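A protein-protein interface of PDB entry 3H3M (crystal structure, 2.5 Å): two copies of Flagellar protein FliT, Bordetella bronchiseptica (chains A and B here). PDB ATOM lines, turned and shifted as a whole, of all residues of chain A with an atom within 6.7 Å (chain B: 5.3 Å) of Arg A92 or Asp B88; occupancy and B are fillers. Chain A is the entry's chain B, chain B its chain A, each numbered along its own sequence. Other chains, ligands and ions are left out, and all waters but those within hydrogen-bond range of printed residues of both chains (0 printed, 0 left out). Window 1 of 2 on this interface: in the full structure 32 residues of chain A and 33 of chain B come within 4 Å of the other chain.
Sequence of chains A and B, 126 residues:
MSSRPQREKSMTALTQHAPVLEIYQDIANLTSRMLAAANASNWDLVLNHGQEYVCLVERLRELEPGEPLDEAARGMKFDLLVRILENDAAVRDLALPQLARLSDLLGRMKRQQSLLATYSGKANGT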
ATOM      1  N   ALA A  38     -34.984 -10.313 -17.599  1.00  0.00           N
ATOM      2  CA  ALA A  38     -33.897 -10.445 -18.573  1.00  0.00           C
ATOM      3  C   ALA A  38     -34.285  -9.744 -19.853  1.00  0.00           C
ATOM      4  O   ALA A  38     -33.595  -8.866 -20.332  1.00  0.00           O
ATOM      5  CB  ALA A  38     -33.641 -11.954 -18.873  1.00  0.00           C
ATOM      6  N   TYR A  53     -34.510 -18.347  -5.885  1.00  0.00           N
ATOM      7  CA  TYR A  53     -34.195 -19.613  -6.583  1.00  0.00           C
ATOM      8  C   TYR A  53     -33.309 -20.506  -5.722  1.00  0.00           C
ATOM      9  O   TYR A  53     -33.654 -21.616  -5.425  1.00  0.00           O
ATOM     10  CB  TYR A  53     -33.480 -19.265  -7.903  1.00  0.00           C
ATOM     11  CG  TYR A  53     -33.063 -20.370  -8.867  1.00  0.00           C
ATOM     12  CD1 TYR A  53     -33.652 -20.464 -10.126  1.00  0.00           C
ATOM     13  CD2 TYR A  53     -32.022 -21.269  -8.561  1.00  0.00           C
ATOM     14  CE1 TYR A  53     -33.226 -21.433 -11.060  1.00  0.00           C
ATOM     15  CE2 TYR A  53     -31.594 -22.247  -9.477  1.00  0.00           C
ATOM     16  CZ  TYR A  53     -32.200 -22.311 -10.728  1.00  0.00           C
ATOM     17  OH  TYR A  53     -31.799 -23.242 -11.650  1.00  0.00           O
ATOM     18  N   ILE A  84     -37.769 -25.009 -16.474  1.00  0.00           N
ATOM     19  CA  ILE A  84     -36.624 -24.432 -15.734  1.00  0.00           C
ATOM     20  C   ILE A  84     -35.294 -24.420 -16.541  1.00  0.00           C
ATOM     21  O   ILE A  84     -34.535 -23.418 -16.576  1.00  0.00           O
ATOM     22  CB  ILE A  84     -36.356 -25.141 -14.396  1.00  0.00           C
ATOM     23  CG1 ILE A  84     -37.525 -24.935 -13.417  1.00  0.00           C
ATOM     24  CG2 ILE A  84     -35.004 -24.646 -13.779  1.00  0.00           C
ATOM     25  CD1 ILE A  84     -37.687 -26.055 -12.375  1.00  0.00           C
ATOM     26  N   LEU A  85     -35.015 -25.554 -17.143  1.00  0.00           N
ATOM     27  CA  LEU A  85     -33.838 -25.742 -17.991  1.00  0.00           C
ATOM     28  C   LEU A  85     -33.834 -24.823 -19.181  1.00  0.00           C
ATOM     29  O   LEU A  85     -32.819 -24.188 -19.453  1.00  0.00           O
ATOM     30  CB  LEU A  85     -33.752 -27.197 -18.442  1.00  0.00           C
ATOM     31  CG  LEU A  85     -33.420 -28.135 -17.258  1.00  0.00           C
ATOM     32  CD1 LEU A  85     -33.225 -29.627 -17.653  1.00  0.00           C
ATOM     33  CD2 LEU A  85     -32.227 -27.624 -16.550  1.00  0.00           C
ATOM     34  N   ASN A  87     -35.451 -21.978 -19.290  1.00  0.00           N
ATOM     35  CA  ASN A  87     -35.444 -20.604 -18.817  1.00  0.00           C
ATOM     36  C   ASN A  87     -34.057 -20.097 -18.452  1.00  0.00           C
ATOM     37  O   ASN A  87     -33.695 -18.962 -18.777  1.00  0.00           O
ATOM     38  CB  ASN A  87     -36.447 -20.409 -17.688  1.00  0.00           C
ATOM     39  CG  ASN A  87     -37.899 -20.338 -18.196  1.00  0.00           C
ATOM     40  OD1 ASN A  87     -38.116 -20.244 -19.375  1.00  0.00           O
ATOM     41  ND2 ASN A  87     -38.874 -20.323 -17.288  1.00  0.00           N
ATOM     42  N   ASP A  88     -33.277 -20.948 -17.812  1.00  0.00           N
ATOM     43  CA  ASP A  88     -31.905 -20.643 -17.431  1.00  0.00           C
ATOM     44  C   ASP A  88     -31.162 -20.403 -18.706  1.00  0.00           C
ATOM     45  O   ASP A  88     -30.436 -19.436 -18.797  1.00  0.00           O
ATOM     46  CB  ASP A  88     -31.282 -21.805 -16.635  1.00  0.00           C
ATOM     47  CG  ASP A  88     -31.893 -21.967 -15.187  1.00  0.00           C
ATOM     48  OD1 ASP A  88     -32.585 -21.036 -14.680  1.00  0.00           O
ATOM     49  OD2 ASP A  88     -31.662 -23.030 -14.534  1.00  0.00           O
ATOM     50  N   ALA A  89     -31.372 -21.246 -19.715  1.00  0.00           N
ATOM     51  CA  ALA A  89     -30.636 -21.101 -20.941  1.00  0.00           C
ATOM     52  C   ALA A  89     -31.075 -19.819 -21.644  1.00  0.00           C
ATOM     53  O   ALA A  89     -30.249 -19.100 -22.182  1.00  0.00           O
ATOM     54  CB  ALA A  89     -30.812 -22.327 -21.849  1.00  0.00           C
ATOM     55  N   ALA A  90     -32.370 -19.518 -21.620  1.00  0.00           N
ATOM     56  CA  ALA A  90     -32.903 -18.311 -22.299  1.00  0.00           C
ATOM     57  C   ALA A  90     -32.349 -17.066 -21.666  1.00  0.00           C
ATOM     58  O   ALA A  90     -31.972 -16.164 -22.367  1.00  0.00           O
ATOM     59  CB  ALA A  90     -34.378 -18.294 -22.308  1.00  0.00           C
ATOM     60  N   VAL A  91     -32.225 -17.022 -20.344  1.00  0.00           N
ATOM     61  CA  VAL A  91     -31.609 -15.869 -19.680  1.00  0.00           C
ATOM     62  C   VAL A  91     -30.114 -15.747 -20.034  1.00  0.00           C
ATOM     63  O   VAL A  91     -29.660 -14.666 -20.388  1.00  0.00           O
ATOM     64  CB  VAL A  91     -31.820 -15.900 -18.163  1.00  0.00           C
ATOM     65  CG1 VAL A  91     -31.112 -14.675 -17.473  1.00  0.00           C
ATOM     66  CG2 VAL A  91     -33.346 -15.935 -17.802  1.00  0.00           C
ATOM     67  N   ARG A  92     -29.343 -16.844 -19.990  1.00  0.00           N
ATOM     68  CA  ARG A  92     -27.935 -16.793 -20.379  1.00  0.00           C
ATOM     69  C   ARG A  92     -27.796 -16.257 -21.795  1.00  0.00           C
ATOM     70  O   ARG A  92     -26.951 -15.432 -22.056  1.00  0.00           O
ATOM     71  CB  ARG A  92     -27.325 -18.198 -20.335  1.00  0.00           C
ATOM     72  CG  ARG A  92     -27.059 -18.734 -18.922  1.00  0.00           C
ATOM     73  CD  ARG A  92     -26.108 -19.938 -18.969  1.00  0.00           C
ATOM     74  NE  ARG A  92     -26.658 -21.093 -19.684  1.00  0.00           N
ATOM     75  CZ  ARG A  92     -27.362 -22.080 -19.137  1.00  0.00           C
ATOM     76  NH1 ARG A  92     -27.618 -22.084 -17.857  1.00  0.00           N
ATOM     77  NH2 ARG A  92     -27.828 -23.076 -19.874  1.00  0.00           N
ATOM     78  N   ASP A  93     -28.617 -16.748 -22.712  1.00  0.00           N
ATOM     79  CA  ASP A  93     -28.598 -16.303 -24.109  1.00  0.00           C
ATOM     80  C   ASP A  93     -28.896 -14.816 -24.322  1.00  0.00           C
ATOM     81  O   ASP A  93     -28.378 -14.232 -25.249  1.00  0.00           O
ATOM     82  CB  ASP A  93     -29.576 -17.167 -24.942  1.00  0.00           C
ATOM     83  CG  ASP A  93     -29.052 -18.606 -25.131  1.00  0.00           C
ATOM     84  OD1 ASP A  93     -27.805 -18.798 -25.035  1.00  0.00           O
ATOM     85  OD2 ASP A  93     -29.866 -19.526 -25.370  1.00  0.00           O
ATOM     86  N   LEU A  94     -29.718 -14.218 -23.467  1.00  0.00           N
ATOM     87  CA  LEU A  94     -29.918 -12.770 -23.463  1.00  0.00           C
ATOM     88  C   LEU A  94     -28.737 -12.078 -22.809  1.00  0.00           C
ATOM     89  O   LEU A  94     -28.149 -11.199 -23.395  1.00  0.00           O
ATOM     90  CB  LEU A  94     -31.192 -12.418 -22.686  1.00  0.00           C
ATOM     91  CG  LEU A  94     -32.479 -12.867 -23.389  1.00  0.00           C
ATOM     92  CD1 LEU A  94     -33.707 -12.805 -22.499  1.00  0.00           C
ATOM     93  CD2 LEU A  94     -32.683 -12.007 -24.695  1.00  0.00           C
ATOM     94  N   ALA A  95     -28.381 -12.485 -21.596  1.00  0.00           N
ATOM     95  CA  ALA A  95     -27.410 -11.748 -20.744  1.00  0.00           C
ATOM     96  C   ALA A  95     -25.975 -11.764 -21.243  1.00  0.00           C
ATOM     97  O   ALA A  95     -25.286 -10.733 -21.188  1.00  0.00           O
ATOM     98  CB  ALA A  95     -27.449 -12.276 -19.296  1.00  0.00           C
ATOM     99  N   LEU A  96     -25.517 -12.922 -21.725  1.00  0.00           N
ATOM    100  CA  LEU A  96     -24.089 -13.119 -21.973  1.00  0.00           C
ATOM    101  C   LEU A  96     -23.500 -12.432 -23.196  1.00  0.00           C
ATOM    102  O   LEU A  96     -22.337 -11.987 -23.148  1.00  0.00           O
ATOM    103  CB  LEU A  96     -23.746 -14.608 -22.022  1.00  0.00           C
ATOM    104  CG  LEU A  96     -24.009 -15.393 -20.728  1.00  0.00           C
ATOM    105  CD1 LEU A  96     -23.431 -16.786 -20.803  1.00  0.00           C
ATOM    106  CD2 LEU A  96     -23.406 -14.622 -19.599  1.00  0.00           C
ATOM    107  N   PRO A  97     -24.262 -12.350 -24.304  1.00  0.00           N
ATOM    108  CA  PRO A  97     -23.638 -11.578 -25.389  1.00  0.00           C
ATOM    109  C   PRO A  97     -23.482 -10.099 -24.992  1.00  0.00           C
ATOM    110  O   PRO A  97     -22.498  -9.472 -25.377  1.00  0.00           O
ATOM    111  CB  PRO A  97     -24.585 -11.778 -26.603  1.00  0.00           C
ATOM    112  CG  PRO A  97     -25.575 -12.886 -26.218  1.00  0.00           C
ATOM    113  CD  PRO A  97     -25.607 -12.826 -24.662  1.00  0.00           C
ATOM    114  N   THR B  31     -22.911 -28.472 -17.275  1.00  0.00           N
ATOM    115  CA  THR B  31     -23.194 -27.287 -16.449  1.00  0.00           C
ATOM    116  C   THR B  31     -22.026 -26.958 -15.520  1.00  0.00           C
ATOM    117  O   THR B  31     -21.813 -25.791 -15.197  1.00  0.00           O
ATOM    118  CB  THR B  31     -24.538 -27.418 -15.678  1.00  0.00           C
ATOM    119  OG1 THR B  31     -24.515 -28.600 -14.871  1.00  0.00           O
ATOM    120  CG2 THR B  31     -25.692 -27.487 -16.642  1.00  0.00           C
ATOM    121  N   MET B  34     -19.721 -25.176 -17.667  1.00  0.00           N
ATOM    122  CA  MET B  34     -20.172 -23.788 -17.852  1.00  0.00           C
ATOM    123  C   MET B  34     -19.741 -22.960 -16.671  1.00  0.00           C
ATOM    124  O   MET B  34     -19.284 -21.829 -16.835  1.00  0.00           O
ATOM    125  CB  MET B  34     -21.664 -23.649 -17.986  1.00  0.00           C
ATOM    126  CG  MET B  34     -22.214 -24.379 -19.103  1.00  0.00           C
ATOM    127  SD  MET B  34     -24.081 -23.837 -19.294  1.00  0.00           S
ATOM    128  CE  MET B  34     -24.807 -24.539 -17.578  1.00  0.00           C
ATOM    129  N   VAL B  46     -18.994 -19.981 -22.169  1.00  0.00           N
ATOM    130  CA  VAL B  46     -20.224 -20.377 -21.474  1.00  0.00           C
ATOM    131  C   VAL B  46     -21.325 -20.524 -22.510  1.00  0.00           C
ATOM    132  O   VAL B  46     -22.029 -21.540 -22.522  1.00  0.00           O
ATOM    133  CB  VAL B  46     -20.650 -19.354 -20.407  1.00  0.00           C
ATOM    134  CG1 VAL B  46     -22.035 -19.658 -19.923  1.00  0.00           C
ATOM    135  CG2 VAL B  46     -19.640 -19.329 -19.258  1.00  0.00           C
ATOM    136  N   LEU B  47     -21.458 -19.516 -23.389  1.00  0.00           N
ATOM    137  CA  LEU B  47     -22.453 -19.550 -24.468  1.00  0.00           C
ATOM    138  C   LEU B  47     -22.222 -20.704 -25.435  1.00  0.00           C
ATOM    139  O   LEU B  47     -23.151 -21.306 -25.924  1.00  0.00           O
ATOM    140  CB  LEU B  47     -22.387 -18.274 -25.299  1.00  0.00           C
ATOM    141  CG  LEU B  47     -23.353 -17.146 -24.958  1.00  0.00           C
ATOM    142  CD1 LEU B  47     -23.160 -16.042 -26.008  1.00  0.00           C
ATOM    143  CD2 LEU B  47     -24.814 -17.618 -24.836  1.00  0.00           C
ATOM    144  N   TYR B  53     -25.756 -28.054 -24.597  1.00  0.00           N
ATOM    145  CA  TYR B  53     -26.797 -28.056 -23.561  1.00  0.00           C
ATOM    146  C   TYR B  53     -28.167 -28.297 -24.144  1.00  0.00           C
ATOM    147  O   TYR B  53     -28.926 -29.059 -23.605  1.00  0.00           O
ATOM    148  CB  TYR B  53     -26.756 -26.729 -22.800  1.00  0.00           C
ATOM    149  CG  TYR B  53     -27.652 -26.587 -21.578  1.00  0.00           C
ATOM    150  CD1 TYR B  53     -27.168 -26.816 -20.272  1.00  0.00           C
ATOM    151  CD2 TYR B  53     -28.973 -26.160 -21.716  1.00  0.00           C
ATOM    152  CE1 TYR B  53     -27.998 -26.636 -19.141  1.00  0.00           C
ATOM    153  CE2 TYR B  53     -29.798 -25.976 -20.598  1.00  0.00           C
ATOM    154  CZ  TYR B  53     -29.306 -26.213 -19.312  1.00  0.00           C
ATOM    155  OH  TYR B  53     -30.158 -26.000 -18.238  1.00  0.00           O
ATOM    156  N   ARG B  83     -27.620 -30.540  -8.460  1.00  0.00           N
ATOM    157  CA  ARG B  83     -26.323 -30.107  -8.983  1.00  0.00           C
ATOM    158  C   ARG B  83     -26.438 -29.228 -10.247  1.00  0.00           C
ATOM    159  O   ARG B  83     -25.704 -28.222 -10.372  1.00  0.00           O
ATOM    160  CB  ARG B  83     -25.455 -31.315  -9.280  1.00  0.00           C
ATOM    161  CG  ARG B  83     -24.097 -30.979  -9.955  1.00  0.00           C
ATOM    162  CD  ARG B  83     -23.160 -29.998  -9.106  1.00  0.00           C
ATOM    163  NE  ARG B  83     -23.005 -30.397  -7.687  1.00  0.00           N
ATOM    164  CZ  ARG B  83     -22.013 -31.155  -7.178  1.00  0.00           C
ATOM    165  NH1 ARG B  83     -21.032 -31.617  -7.949  1.00  0.00           N
ATOM    166  NH2 ARG B  83     -21.993 -31.447  -5.877  1.00  0.00           N
ATOM    167  N   ILE B  84     -27.321 -29.623 -11.175  1.00  0.00           N
ATOM    168  CA  ILE B  84     -27.537 -28.859 -12.417  1.00  0.00           C
ATOM    169  C   ILE B  84     -28.121 -27.496 -12.073  1.00  0.00           C
ATOM    170  O   ILE B  84     -27.688 -26.465 -12.581  1.00  0.00           O
ATOM    171  CB  ILE B  84     -28.559 -29.570 -13.362  1.00  0.00           C
ATOM    172  CG1 ILE B  84     -28.031 -30.902 -13.915  1.00  0.00           C
ATOM    173  CG2 ILE B  84     -28.981 -28.683 -14.532  1.00  0.00           C
ATOM    174  CD1 ILE B  84     -29.149 -31.811 -14.433  1.00  0.00           C
ATOM    175  N   LEU B  85     -29.149 -27.488 -11.236  1.00  0.00           N
ATOM    176  CA  LEU B  85     -29.737 -26.229 -10.818  1.00  0.00           C
ATOM    177  C   LEU B  85     -28.722 -25.340 -10.053  1.00  0.00           C
ATOM    178  O   LEU B  85     -28.640 -24.140 -10.305  1.00  0.00           O
ATOM    179  CB  LEU B  85     -30.991 -26.468  -9.982  1.00  0.00           C
ATOM    180  CG  LEU B  85     -32.213 -27.161 -10.655  1.00  0.00           C
ATOM    181  CD1 LEU B  85     -33.347 -27.420  -9.606  1.00  0.00           C
ATOM    182  CD2 LEU B  85     -32.733 -26.439 -11.913  1.00  0.00           C
ATOM    183  N   GLU B  86     -27.969 -25.909  -9.114  1.00  0.00           N
ATOM    184  CA  GLU B  86     -26.943 -25.146  -8.383  1.00  0.00           C
ATOM    185  C   GLU B  86     -25.901 -24.541  -9.336  1.00  0.00           C
ATOM    186  O   GLU B  86     -25.434 -23.404  -9.160  1.00  0.00           O
ATOM    187  CB  GLU B  86     -26.200 -26.033  -7.384  1.00  0.00           C
ATOM    188  CG  GLU B  86     -26.928 -26.352  -6.112  1.00  0.00           C
ATOM    189  CD  GLU B  86     -26.058 -27.159  -5.119  1.00  0.00           C
ATOM    190  OE1 GLU B  86     -25.062 -27.799  -5.546  1.00  0.00           O
ATOM    191  OE2 GLU B  86     -26.394 -27.139  -3.908  1.00  0.00           O
ATOM    192  N   ASN B  87     -25.533 -25.308 -10.352  1.00  0.00           N
ATOM    193  CA  ASN B  87     -24.603 -24.810 -11.365  1.00  0.00           C
ATOM    194  C   ASN B  87     -25.157 -23.683 -12.185  1.00  0.00           C
ATOM    195  O   ASN B  87     -24.468 -22.689 -12.453  1.00  0.00           O
ATOM    196  CB  ASN B  87     -24.141 -25.945 -12.251  1.00  0.00           C
ATOM    197  CG  ASN B  87     -23.089 -26.779 -11.596  1.00  0.00           C
ATOM    198  OD1 ASN B  87     -22.456 -26.344 -10.606  1.00  0.00           O
ATOM    199  ND2 ASN B  87     -22.862 -27.994 -12.143  1.00  0.00           N
ATOM    200  N   ASP B  88     -26.417 -23.804 -12.530  1.00  0.00           N
ATOM    201  CA  ASP B  88     -27.118 -22.790 -13.293  1.00  0.00           C
ATOM    202  C   ASP B  88     -27.166 -21.516 -12.472  1.00  0.00           C
ATOM    203  O   ASP B  88     -26.858 -20.427 -12.963  1.00  0.00           O
ATOM    204  CB  ASP B  88     -28.521 -23.300 -13.639  1.00  0.00           C
ATOM    205  CG  ASP B  88     -28.582 -24.070 -14.988  1.00  0.00           C
ATOM    206  OD1 ASP B  88     -27.514 -24.414 -15.529  1.00  0.00           O
ATOM    207  OD2 ASP B  88     -29.713 -24.288 -15.542  1.00  0.00           O
ATOM    208  N   ALA B  89     -27.514 -21.646 -11.193  1.00  0.00           N
ATOM    209  CA  ALA B  89     -27.584 -20.462 -10.299  1.00  0.00           C
ATOM    210  C   ALA B  89     -26.213 -19.802 -10.144  1.00  0.00           C
ATOM    211  O   ALA B  89     -26.093 -18.586 -10.144  1.00  0.00           O
ATOM    212  CB  ALA B  89     -28.151 -20.836  -8.959  1.00  0.00           C
ATOM    213  N   ALA B  90     -25.179 -20.632 -10.026  1.00  0.00           N
ATOM    214  CA  ALA B  90     -23.827 -20.154  -9.740  1.00  0.00           C
ATOM    215  C   ALA B  90     -23.285 -19.349 -10.944  1.00  0.00           C
ATOM    216  O   ALA B  90     -22.637 -18.323 -10.747  1.00  0.00           O
ATOM    217  CB  ALA B  90     -22.910 -21.301  -9.341  1.00  0.00           C
ATOM    218  N   VAL B  91     -23.583 -19.795 -12.167  1.00  0.00           N
ATOM    219  CA  VAL B  91     -23.209 -19.054 -13.404  1.00  0.00           C
ATOM    220  C   VAL B  91     -23.835 -17.659 -13.413  1.00  0.00           C
ATOM    221  O   VAL B  91     -23.173 -16.644 -13.625  1.00  0.00           O
ATOM    222  CB  VAL B  91     -23.590 -19.835 -14.754  1.00  0.00           C
ATOM    223  CG1 VAL B  91     -23.481 -18.902 -15.956  1.00  0.00           C
ATOM    224  CG2 VAL B  91     -22.661 -21.109 -15.017  1.00  0.00           C
ATOM    225  N   ARG B  92     -25.119 -17.616 -13.160  1.00  0.00           N
ATOM    226  CA  ARG B  92     -25.832 -16.373 -13.112  1.00  0.00           C
ATOM    227  C   ARG B  92     -25.238 -15.451 -12.038  1.00  0.00           C
ATOM    228  O   ARG B  92     -25.118 -14.241 -12.226  1.00  0.00           O
ATOM    229  CB  ARG B  92     -27.247 -16.730 -12.755  1.00  0.00           C
ATOM    230  CG  ARG B  92     -28.289 -15.716 -12.956  1.00  0.00           C
ATOM    231  CD  ARG B  92     -29.591 -16.449 -13.241  1.00  0.00           C
ATOM    232  NE  ARG B  92     -29.971 -17.205 -12.077  1.00  0.00           N
ATOM    233  CZ  ARG B  92     -30.589 -18.391 -12.082  1.00  0.00           C
ATOM    234  NH1 ARG B  92     -30.907 -19.001 -13.234  1.00  0.00           N
ATOM    235  NH2 ARG B  92     -30.905 -18.956 -10.904  1.00  0.00           N
ATOM    236  N   ASP B  93     -24.875 -16.027 -10.898  1.00  0.00           N
ATOM    237  CA  ASP B  93     -24.417 -15.244  -9.757  1.00  0.00           C
ATOM    238  C   ASP B  93     -22.979 -14.747  -9.966  1.00  0.00           C
ATOM    239  O   ASP B  93     -22.492 -13.938  -9.189  1.00  0.00           O
ATOM    240  CB  ASP B  93     -24.470 -16.079  -8.465  1.00  0.00           C
ATOM    241  CG  ASP B  93     -25.867 -16.096  -7.797  1.00  0.00           C
ATOM    242  OD1 ASP B  93     -26.775 -15.400  -8.296  1.00  0.00           O
ATOM    243  OD2 ASP B  93     -26.054 -16.811  -6.781  1.00  0.00           O
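NH1 of Arg B92 lies within salt-bridge range of OD1 of Asp A88 (3.0 Å).
OD2 of Asp B88 sits close to OD2 of Asp A88 (2.5 Å).
OD1 of Asp B88 lies within salt-bridge range of NH1 of Arg A92 (3.3 Å).
OH of Tyr B53 lies close to O of Leu A85, at 3.4 Å.
SD of Met B34 sits close to NE of Arg A92, at 3.8 Å.
The side-chain carboxylate (OD2) of Asp B88 is in hydrogen-bond range of the side-chain hydroxyl (OH) of Tyr B53, at 3.2 Å.
The side-chain hydroxyl (OH) of Tyr A53 lies within hydrogen-bond range of the side-chain carboxylate (OD2) of Asp A88, at 2.9 Å.
Tyr A53 touches Leu B85.
CB of Ala B89 touches CE2 of Tyr A53, 3.8 Å away.
Arg B92 touches Tyr A53 (NH2 to CD1, 3.2 Å).
Leu B85 touches Ile A84 (CD2 to CG2, 3.4 Å).
Leu A85 touches Ile B84.
Ala A89 touches Tyr B53 (CB to CE2, 3.99 Å).
Arg A92 touches Tyr B53 (NH2 to CZ, 3.5 Å).
Leu A96 touches Val B46.
CB of Leu A96 touches CG of Leu B47 (3.9 Å).
Pro A97 touches Leu B47 (CG to CD1, 3.98 Å).
Of the printed residues of chain B, Leu A85 touches Tyr B53 (3.1 Å) and Ile B84 (3.97 Å).
Of the printed residues of chain B, Ala A89 touches Tyr B53 (3.99 Å).
Val A91 touches none of the printed residues of chain B.
Arg A92 touches just these residues of chain B: Met B34, Tyr B53 and Asp B88.
Of the printed residues of chain A, Met B34 touches Arg A92.
Of the printed residues of chain A, Val B46 touches Leu A96.
Of the printed residues of chain A, Ile B84 touches Leu A85 (3.97 Å).
Asn B87 touches none of the printed residues of chain A.
Of chain A, only Tyr A53, Asp A88 and Arg A92 come within 4 Å of Asp B88.
The nearest printed residue of chain B that does not touch Asp A93 is Val B46 (6.9 Å).
Printed residues of chain A that touch a printed residue of chain B: Tyr A53, Ile A84, Leu A85, Asp A88, Ala A89, Arg A92, Asp A93, Leu A96 and Pro A97.
Of the 16 printed residues of chain B, 9 touch a printed residue of chain A.
Printed residues of chain B that touch a printed residue of chain A: Met B34, Val B46, Leu B47, Tyr B53, Ile B84, Leu B85, Asp B88, Ala B89 and Arg B92.
Hydrophobic or aromatic side chains of chain B within 4 Å of the printed part of chain A: Met B34, Val B46, Leu B47, Tyr B53, Ile B84, Leu B85 and Ala B89.
Among the printed residues, Asp or Glu carboxylates within 4 Å of a Lys or Arg side-chain nitrogen of the other chain: Asp A88 with Arg B92 (3.0 Å) and Arg A92 with Asp B88 (3.3 Å).
Tyr A53 touches Asp B88, but with the chains exchanged Asp A88 does not touch Tyr B53 (4.6 Å).
Tyr A53 touches Ala B89, and with the chains exchanged Ala A89 touches Tyr B53.
Tyr A53 touches Arg B92, and with the chains exchanged Arg A92 touches Tyr B53.
Asp A88 touches Arg B92, and with the chains exchanged Arg A92 touches Asp B88.
Positions printed for both chains: 53, 84, 85, 87, 88, 89, 90, 91, 92 and 93.
Of the 17 pairs that touch across the chains among the printed residues, 11 have their exchanged pair printed and touching as well.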
